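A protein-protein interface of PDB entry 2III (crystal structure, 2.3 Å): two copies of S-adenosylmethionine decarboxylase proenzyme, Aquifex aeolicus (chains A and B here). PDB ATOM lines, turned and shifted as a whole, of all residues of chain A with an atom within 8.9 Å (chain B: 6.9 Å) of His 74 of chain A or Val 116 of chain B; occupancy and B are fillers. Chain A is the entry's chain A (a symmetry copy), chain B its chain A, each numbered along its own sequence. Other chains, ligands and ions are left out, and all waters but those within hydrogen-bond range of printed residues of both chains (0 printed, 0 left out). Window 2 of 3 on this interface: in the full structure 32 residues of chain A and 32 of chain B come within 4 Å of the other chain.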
ATOM      1  N   LEU A  13       4.171   6.959   8.604  1.00  0.00           N
ATOM      2  CA  LEU A  13       4.504   7.956   9.614  1.00  0.00           C
ATOM      3  C   LEU A  13       5.255   7.356  10.798  1.00  0.00           C
ATOM      4  O   LEU A  13       4.772   6.424  11.435  1.00  0.00           O
ATOM      5  CB  LEU A  13       3.220   8.629  10.107  1.00  0.00           C
ATOM      6  CG  LEU A  13       2.148   8.966   9.066  1.00  0.00           C
ATOM      7  CD1 LEU A  13       1.033   9.726   9.757  1.00  0.00           C
ATOM      8  CD2 LEU A  13       2.727   9.798   7.927  1.00  0.00           C
ATOM      9  N   TYR A  14       6.431   7.908  11.092  1.00  0.00           N
ATOM     10  CA  TYR A  14       7.259   7.432  12.195  1.00  0.00           C
ATOM     11  C   TYR A  14       7.380   8.462  13.316  1.00  0.00           C
ATOM     12  O   TYR A  14       7.167   9.658  13.115  1.00  0.00           O
ATOM     13  CB  TYR A  14       8.666   7.088  11.699  1.00  0.00           C
ATOM     14  CG  TYR A  14       8.711   6.041  10.606  1.00  0.00           C
ATOM     15  CD1 TYR A  14       9.249   4.778  10.851  1.00  0.00           C
ATOM     16  CD2 TYR A  14       8.231   6.318   9.321  1.00  0.00           C
ATOM     17  CE1 TYR A  14       9.313   3.823   9.854  1.00  0.00           C
ATOM     18  CE2 TYR A  14       8.291   5.359   8.307  1.00  0.00           C
ATOM     19  CZ  TYR A  14       8.836   4.113   8.587  1.00  0.00           C
ATOM     20  OH  TYR A  14       8.916   3.152   7.607  1.00  0.00           O
ATOM     21  N   GLY A  15       7.737   7.986  14.503  1.00  0.00           N
ATOM     22  CA  GLY A  15       7.895   8.886  15.629  1.00  0.00           C
ATOM     23  C   GLY A  15       6.569   9.381  16.157  1.00  0.00           C
ATOM     24  O   GLY A  15       6.500  10.437  16.778  1.00  0.00           O
ATOM     25  N   VAL A  16       5.512   8.615  15.910  1.00  0.00           N
ATOM     26  CA  VAL A  16       4.184   8.987  16.377  1.00  0.00           C
ATOM     27  C   VAL A  16       3.962   8.487  17.804  1.00  0.00           C
ATOM     28  O   VAL A  16       4.203   7.316  18.101  1.00  0.00           O
ATOM     29  CB  VAL A  16       3.085   8.387  15.480  1.00  0.00           C
ATOM     30  CG1 VAL A  16       1.708   8.683  16.082  1.00  0.00           C
ATOM     31  CG2 VAL A  16       3.203   8.951  14.057  1.00  0.00           C
ATOM     32  N   ASP A  17       3.508   9.372  18.686  1.00  0.00           N
ATOM     33  CA  ASP A  17       3.253   8.984  20.071  1.00  0.00           C
ATOM     34  C   ASP A  17       2.295   7.790  20.099  1.00  0.00           C
ATOM     35  O   ASP A  17       1.265   7.784  19.412  1.00  0.00           O
ATOM     36  CB  ASP A  17       2.666  10.169  20.851  1.00  0.00           C
ATOM     37  CG  ASP A  17       3.656  11.312  21.004  1.00  0.00           C
ATOM     38  OD1 ASP A  17       3.231  12.444  21.327  1.00  0.00           O
ATOM     39  OD2 ASP A  17       4.867  11.076  20.808  1.00  0.00           O
ATOM     40  N   ALA A  18       2.657   6.778  20.883  1.00  0.00           N
ATOM     41  CA  ALA A  18       1.873   5.551  21.023  1.00  0.00           C
ATOM     42  C   ALA A  18       0.439   5.802  21.478  1.00  0.00           C
ATOM     43  O   ALA A  18      -0.469   5.076  21.093  1.00  0.00           O
ATOM     44  CB  ALA A  18       2.561   4.604  22.011  1.00  0.00           C
ATOM     45  N   ILE A  21      -2.243   6.502  18.661  1.00  0.00           N
ATOM     46  CA  ILE A  21      -2.598   5.429  17.736  1.00  0.00           C
ATOM     47  C   ILE A  21      -2.762   4.040  18.345  1.00  0.00           C
ATOM     48  O   ILE A  21      -2.637   3.042  17.632  1.00  0.00           O
ATOM     49  CB  ILE A  21      -1.513   5.317  16.634  1.00  0.00           C
ATOM     50  CG1 ILE A  21      -0.146   5.110  17.294  1.00  0.00           C
ATOM     51  CG2 ILE A  21      -1.495   6.585  15.771  1.00  0.00           C
ATOM     52  CD1 ILE A  21       1.037   4.974  16.326  1.00  0.00           C
ATOM     53  N   HIS A  53      -2.673  -3.880  21.393  1.00  0.00           N
ATOM     54  CA  HIS A  53      -2.970  -2.518  20.970  1.00  0.00           C
ATOM     55  C   HIS A  53      -2.788  -2.369  19.466  1.00  0.00           C
ATOM     56  O   HIS A  53      -2.351  -3.299  18.783  1.00  0.00           O
ATOM     57  CB  HIS A  53      -2.076  -1.517  21.708  1.00  0.00           C
ATOM     58  CG  HIS A  53      -0.627  -1.896  21.735  1.00  0.00           C
ATOM     59  ND1 HIS A  53       0.076  -2.242  20.599  1.00  0.00           N
ATOM     60  CD2 HIS A  53       0.263  -1.942  22.755  1.00  0.00           C
ATOM     61  CE1 HIS A  53       1.335  -2.481  20.919  1.00  0.00           C
ATOM     62  NE2 HIS A  53       1.476  -2.306  22.221  1.00  0.00           N
ATOM     63  N   THR A  70      -1.954   0.679  12.380  1.00  0.00           N
ATOM     64  CA  THR A  70      -0.993   1.201  13.345  1.00  0.00           C
ATOM     65  C   THR A  70      -0.266   0.183  14.213  1.00  0.00           C
ATOM     66  O   THR A  70      -0.746  -0.926  14.438  1.00  0.00           O
ATOM     67  CB  THR A  70      -1.658   2.226  14.281  1.00  0.00           C
ATOM     68  OG1 THR A  70      -2.466   1.539  15.245  1.00  0.00           O
ATOM     69  CG2 THR A  70      -2.540   3.174  13.485  1.00  0.00           C
ATOM     70  N   TRP A  71       0.897   0.603  14.702  1.00  0.00           N
ATOM     71  CA  TRP A  71       1.762  -0.207  15.550  1.00  0.00           C
ATOM     72  C   TRP A  71       2.315   0.712  16.622  1.00  0.00           C
ATOM     73  O   TRP A  71       3.356   1.344  16.436  1.00  0.00           O
ATOM     74  CB  TRP A  71       2.929  -0.780  14.742  1.00  0.00           C
ATOM     75  CG  TRP A  71       2.538  -1.830  13.749  1.00  0.00           C
ATOM     76  CD1 TRP A  71       2.588  -3.180  13.927  1.00  0.00           C
ATOM     77  CD2 TRP A  71       2.035  -1.613  12.422  1.00  0.00           C
ATOM     78  NE1 TRP A  71       2.150  -3.821  12.790  1.00  0.00           N
ATOM     79  CE2 TRP A  71       1.804  -2.886  11.854  1.00  0.00           C
ATOM     80  CE3 TRP A  71       1.760  -0.468  11.658  1.00  0.00           C
ATOM     81  CZ2 TRP A  71       1.306  -3.049  10.550  1.00  0.00           C
ATOM     82  CZ3 TRP A  71       1.267  -0.629  10.361  1.00  0.00           C
ATOM     83  CH2 TRP A  71       1.045  -1.915   9.823  1.00  0.00           C
ATOM     84  N   PRO A  72       1.603   0.828  17.748  1.00  0.00           N
ATOM     85  CA  PRO A  72       2.038   1.682  18.850  1.00  0.00           C
ATOM     86  C   PRO A  72       3.489   1.422  19.277  1.00  0.00           C
ATOM     87  O   PRO A  72       4.247   2.363  19.508  1.00  0.00           O
ATOM     88  CB  PRO A  72       1.039   1.336  19.950  1.00  0.00           C
ATOM     89  CG  PRO A  72      -0.221   1.138  19.173  1.00  0.00           C
ATOM     90  CD  PRO A  72       0.248   0.302  17.997  1.00  0.00           C
ATOM     91  N   GLU A  73       3.876   0.150  19.371  1.00  0.00           N
ATOM     92  CA  GLU A  73       5.228  -0.196  19.816  1.00  0.00           C
ATOM     93  C   GLU A  73       6.321   0.356  18.913  1.00  0.00           C
ATOM     94  O   GLU A  73       7.472   0.459  19.332  1.00  0.00           O
ATOM     95  CB  GLU A  73       5.403  -1.717  19.930  1.00  0.00           C
ATOM     96  CG  GLU A  73       5.453  -2.450  18.584  1.00  0.00           C
ATOM     97  CD  GLU A  73       4.083  -2.886  18.081  1.00  0.00           C
ATOM     98  OE1 GLU A  73       3.118  -2.098  18.195  1.00  0.00           O
ATOM     99  OE2 GLU A  73       3.981  -4.019  17.561  1.00  0.00           O
ATOM    100  N   HIS A  74       5.960   0.703  17.677  1.00  0.00           N
ATOM    101  CA  HIS A  74       6.917   1.243  16.712  1.00  0.00           C
ATOM    102  C   HIS A  74       6.667   2.713  16.399  1.00  0.00           C
ATOM    103  O   HIS A  74       7.352   3.290  15.549  1.00  0.00           O
ATOM    104  CB  HIS A  74       6.869   0.443  15.409  1.00  0.00           C
ATOM    105  CG  HIS A  74       7.386  -0.956  15.538  1.00  0.00           C
ATOM    106  ND1 HIS A  74       6.600  -2.067  15.313  1.00  0.00           N
ATOM    107  CD2 HIS A  74       8.608  -1.425  15.879  1.00  0.00           C
ATOM    108  CE1 HIS A  74       7.316  -3.159  15.509  1.00  0.00           C
ATOM    109  NE2 HIS A  74       8.537  -2.794  15.853  1.00  0.00           N
ATOM    110  N   GLY A  75       5.700   3.318  17.085  1.00  0.00           N
ATOM    111  CA  GLY A  75       5.386   4.714  16.830  1.00  0.00           C
ATOM    112  C   GLY A  75       5.094   4.885  15.353  1.00  0.00           C
ATOM    113  O   GLY A  75       5.378   5.926  14.753  1.00  0.00           O
ATOM    114  N   LEU A  76       4.494   3.856  14.770  1.00  0.00           N
ATOM    115  CA  LEU A  76       4.209   3.852  13.344  1.00  0.00           C
ATOM    116  C   LEU A  76       2.755   3.712  12.937  1.00  0.00           C
ATOM    117  O   LEU A  76       1.985   2.952  13.540  1.00  0.00           O
ATOM    118  CB  LEU A  76       5.005   2.729  12.677  1.00  0.00           C
ATOM    119  CG  LEU A  76       4.629   2.403  11.228  1.00  0.00           C
ATOM    120  CD1 LEU A  76       5.165   3.487  10.317  1.00  0.00           C
ATOM    121  CD2 LEU A  76       5.188   1.040  10.838  1.00  0.00           C
ATOM    122  N   ALA A  77       2.408   4.443  11.880  1.00  0.00           N
ATOM    123  CA  ALA A  77       1.072   4.413  11.299  1.00  0.00           C
ATOM    124  C   ALA A  77       1.227   4.485   9.779  1.00  0.00           C
ATOM    125  O   ALA A  77       1.937   5.343   9.262  1.00  0.00           O
ATOM    126  CB  ALA A  77       0.243   5.600  11.803  1.00  0.00           C
ATOM    127  N   LYS A 104       7.498  12.396  13.505  1.00  0.00           N
ATOM    128  CA  LYS A 104       8.821  13.009  13.467  1.00  0.00           C
ATOM    129  C   LYS A 104       9.501  12.795  12.108  1.00  0.00           C
ATOM    130  O   LYS A 104      10.262  13.647  11.652  1.00  0.00           O
ATOM    131  CB  LYS A 104       9.692  12.452  14.601  1.00  0.00           C
ATOM    132  CG  LYS A 104       9.205  12.881  15.985  1.00  0.00           C
ATOM    133  CD  LYS A 104      10.133  12.425  17.094  1.00  0.00           C
ATOM    134  CE  LYS A 104      10.198  10.908  17.202  1.00  0.00           C
ATOM    135  NZ  LYS A 104      11.181  10.473  18.237  1.00  0.00           N
ATOM    136  N   ALA B   2      17.243  -4.725   9.489  1.00  0.00           N
ATOM    137  CA  ALA B   2      15.930  -4.045   9.315  1.00  0.00           C
ATOM    138  C   ALA B   2      14.967  -4.925   8.524  1.00  0.00           C
ATOM    139  O   ALA B   2      15.358  -5.582   7.555  1.00  0.00           O
ATOM    140  CB  ALA B   2      16.129  -2.717   8.606  1.00  0.00           C
ATOM    141  N   LYS B   3      13.708  -4.942   8.948  1.00  0.00           N
ATOM    142  CA  LYS B   3      12.682  -5.733   8.280  1.00  0.00           C
ATOM    143  C   LYS B   3      11.480  -4.848   7.976  1.00  0.00           C
ATOM    144  O   LYS B   3      11.292  -3.797   8.596  1.00  0.00           O
ATOM    145  CB  LYS B   3      12.239  -6.893   9.176  1.00  0.00           C
ATOM    146  CG  LYS B   3      11.476  -6.455  10.429  1.00  0.00           C
ATOM    147  CD  LYS B   3      11.035  -7.643  11.285  1.00  0.00           C
ATOM    148  CE  LYS B   3      10.012  -8.535  10.575  1.00  0.00           C
ATOM    149  NZ  LYS B   3       8.698  -7.863  10.349  1.00  0.00           N
ATOM    150  N   THR B   4      10.666  -5.276   7.019  1.00  0.00           N
ATOM    151  CA  THR B   4       9.476  -4.523   6.653  1.00  0.00           C
ATOM    152  C   THR B   4       8.292  -5.185   7.358  1.00  0.00           C
ATOM    153  O   THR B   4       8.237  -6.408   7.470  1.00  0.00           O
ATOM    154  CB  THR B   4       9.265  -4.509   5.102  1.00  0.00           C
ATOM    155  OG1 THR B   4       8.156  -3.662   4.774  1.00  0.00           O
ATOM    156  CG2 THR B   4       9.003  -5.910   4.570  1.00  0.00           C
ATOM    157  N   LEU B   5       7.367  -4.374   7.859  1.00  0.00           N
ATOM    158  CA  LEU B   5       6.205  -4.893   8.569  1.00  0.00           C
ATOM    159  C   LEU B   5       5.119  -5.340   7.611  1.00  0.00           C
ATOM    160  O   LEU B   5       4.257  -6.144   7.974  1.00  0.00           O
ATOM    161  CB  LEU B   5       5.640  -3.834   9.524  1.00  0.00           C
ATOM    162  CG  LEU B   5       6.461  -3.560  10.788  1.00  0.00           C
ATOM    163  CD1 LEU B   5       5.867  -2.384  11.544  1.00  0.00           C
ATOM    164  CD2 LEU B   5       6.493  -4.813  11.666  1.00  0.00           C
ATOM    165  N   GLY B 114       6.538   0.465   6.297  1.00  0.00           N
ATOM    166  CA  GLY B 114       7.001   0.397   7.674  1.00  0.00           C
ATOM    167  C   GLY B 114       8.277  -0.381   7.898  1.00  0.00           C
ATOM    168  O   GLY B 114       8.254  -1.608   8.034  1.00  0.00           O
ATOM    169  N   ILE B 115       9.391   0.337   7.955  1.00  0.00           N
ATOM    170  CA  ILE B 115      10.689  -0.289   8.163  1.00  0.00           C
ATOM    171  C   ILE B 115      11.138  -0.113   9.609  1.00  0.00           C
ATOM    172  O   ILE B 115      11.241   1.009  10.108  1.00  0.00           O
ATOM    173  CB  ILE B 115      11.734   0.299   7.200  1.00  0.00           C
ATOM    174  CG1 ILE B 115      11.272   0.059   5.756  1.00  0.00           C
ATOM    175  CG2 ILE B 115      13.097  -0.358   7.432  1.00  0.00           C
ATOM    176  CD1 ILE B 115      12.279   0.476   4.705  1.00  0.00           C
ATOM    177  N   VAL B 116      11.390  -1.236  10.277  1.00  0.00           N
ATOM    178  CA  VAL B 116      11.806  -1.220  11.673  1.00  0.00           C
ATOM    179  C   VAL B 116      13.102  -2.000  11.906  1.00  0.00           C
ATOM    180  O   VAL B 116      13.396  -2.970  11.202  1.00  0.00           O
ATOM    181  CB  VAL B 116      10.689  -1.794  12.587  1.00  0.00           C
ATOM    182  CG1 VAL B 116       9.425  -0.962  12.445  1.00  0.00           C
ATOM    183  CG2 VAL B 116      10.394  -3.237  12.217  1.00  0.00           C
ATOM    184  N   GLU B 117      13.867  -1.562  12.902  1.00  0.00           N
ATOM    185  CA  GLU B 117      15.139  -2.179  13.256  1.00  0.00           C
ATOM    186  C   GLU B 117      14.983  -3.594  13.809  1.00  0.00           C
ATOM    187  O   GLU B 117      13.960  -3.924  14.402  1.00  0.00           O
ATOM    188  CB  GLU B 117      15.869  -1.318  14.294  1.00  0.00           C
ATOM    189  CG  GLU B 117      16.277   0.085  13.821  1.00  0.00           C
ATOM    190  CD  GLU B 117      17.178   0.063  12.591  1.00  0.00           C
ATOM    191  OE1 GLU B 117      17.831  -0.976  12.343  1.00  0.00           O
ATOM    192  OE2 GLU B 117      17.243   1.092  11.878  1.00  0.00           O
ATOM    193  N   GLU B 118      16.008  -4.420  13.597  1.00  0.00           N
ATOM    194  CA  GLU B 118      16.034  -5.801  14.084  1.00  0.00           C
ATOM    195  C   GLU B 118      16.962  -5.852  15.302  1.00  0.00           C
ATOM    196  O   GLU B 118      16.869  -6.746  16.146  1.00  0.00           O
ATOM    197  CB  GLU B 118      16.532  -6.742  12.982  1.00  0.00           C
ATOM    198  CG  GLU B 118      15.590  -6.828  11.782  1.00  0.00           C
ATOM    199  CD  GLU B 118      16.107  -7.730  10.673  1.00  0.00           C
ATOM    200  OE1 GLU B 118      17.103  -7.361  10.013  1.00  0.00           O
ATOM    201  OE2 GLU B 118      15.516  -8.811  10.465  1.00  0.00           O
ATOM    202  N   GLU B 119      17.866  -4.881  15.372  1.00  0.00           N
ATOM    203  CA  GLU B 119      18.793  -4.753  16.488  1.00  0.00           C
ATOM    204  C   GLU B 119      18.371  -3.468  17.158  1.00  0.00           C
ATOM    205  O   GLU B 119      17.911  -2.546  16.495  1.00  0.00           O
ATOM    206  CB  GLU B 119      20.243  -4.596  16.013  1.00  0.00           C
ATOM    207  CG  GLU B 119      20.898  -5.857  15.485  1.00  0.00           C
ATOM    208  CD  GLU B 119      20.258  -6.357  14.210  1.00  0.00           C
ATOM    209  OE1 GLU B 119      20.250  -5.602  13.213  1.00  0.00           O
ATOM    210  OE2 GLU B 119      19.763  -7.506  14.204  1.00  0.00           O
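OH of Tyr 14 of chain A sits at hydrogen-bond distance from N of Ile 115 of chain B (2.9 Å).
The backbone NH (N) of Trp 71 of chain A is in hydrogen-bond range of the backbone carbonyl oxygen (O) of Leu 76 of chain A (2.8 Å). O of Tyr 14 of chain A lies within hydrogen-bond range of N of Lys 104 of chain A (2.8 Å). The backbone NH (N) of Lys 3 of chain B lies within hydrogen-bond range of the backbone carbonyl oxygen (O) of Val 116 of chain B, 3.0 Å away. The backbone NH (N) of Leu 5 of chain B lies within hydrogen-bond range of the backbone carbonyl oxygen (O) of Gly 114 of chain B, 2.9 Å away.
CA of Gly 114 of chain B touches OH of Tyr 14 of chain A (3.4 Å). ND1 of His 74 of chain A touches CD1 of Leu 5 of chain B (3.9 Å). His 74 of chain A touches Val 116 of chain B. Leu 76 of chain A touches Leu 5 of chain B (CD2 to CD1, 3.6 Å). CD2 of Leu 76 of chain A touches CA of Gly 114 of chain B, 3.7 Å away.
Leu 13 of chain A touches none of the printed residues of chain B. Of the printed residues of chain B, Tyr 14 of chain A touches Gly 114 and Ile 115. Asp 17 of chain A touches none of the printed residues of chain B. His 74 of chain A touches just these residues of chain B: Leu 5 (3.9 Å) and Val 116 (3.6 Å). Of the printed residues of chain B, Leu 76 of chain A touches Leu 5 (3.6 Å) and Gly 114 (3.7 Å). Of the printed residues of chain A, Leu 5 of chain B touches His 74 and Leu 76. Of the printed residues of chain A, Ile 115 of chain B touches Tyr 14. Val 116 of chain B touches one residue of chain A. The nearest residue of chain B that does not touch His 74 of chain A is Glu 117 of chain B (5.7 Å). The nearest residue of chain A that does not touch Val 116 of chain B is Leu 76 of chain A (5.0 Å). The nearest printed residue of chain B that does not touch Tyr 14 of chain A is Val 116 of chain B (5.4 Å).
Hydrophobic or aromatic side chains of chain A within 4 Å of the printed part of chain B: Tyr 14, His 74 and Leu 76. Hydrophobic or aromatic side chains of chain B within 4 Å of the printed part of chain A: Leu 5 and Val 116. Among the printed residues, no Asp or Glu carboxylate lies within 4 Å of a Lys or Arg side-chain nitrogen of the other chain.
No position is printed for both chains. Of the 6 pairs that touch across the chains among the printed residues, none has its exchanged pair printed and touching as well.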
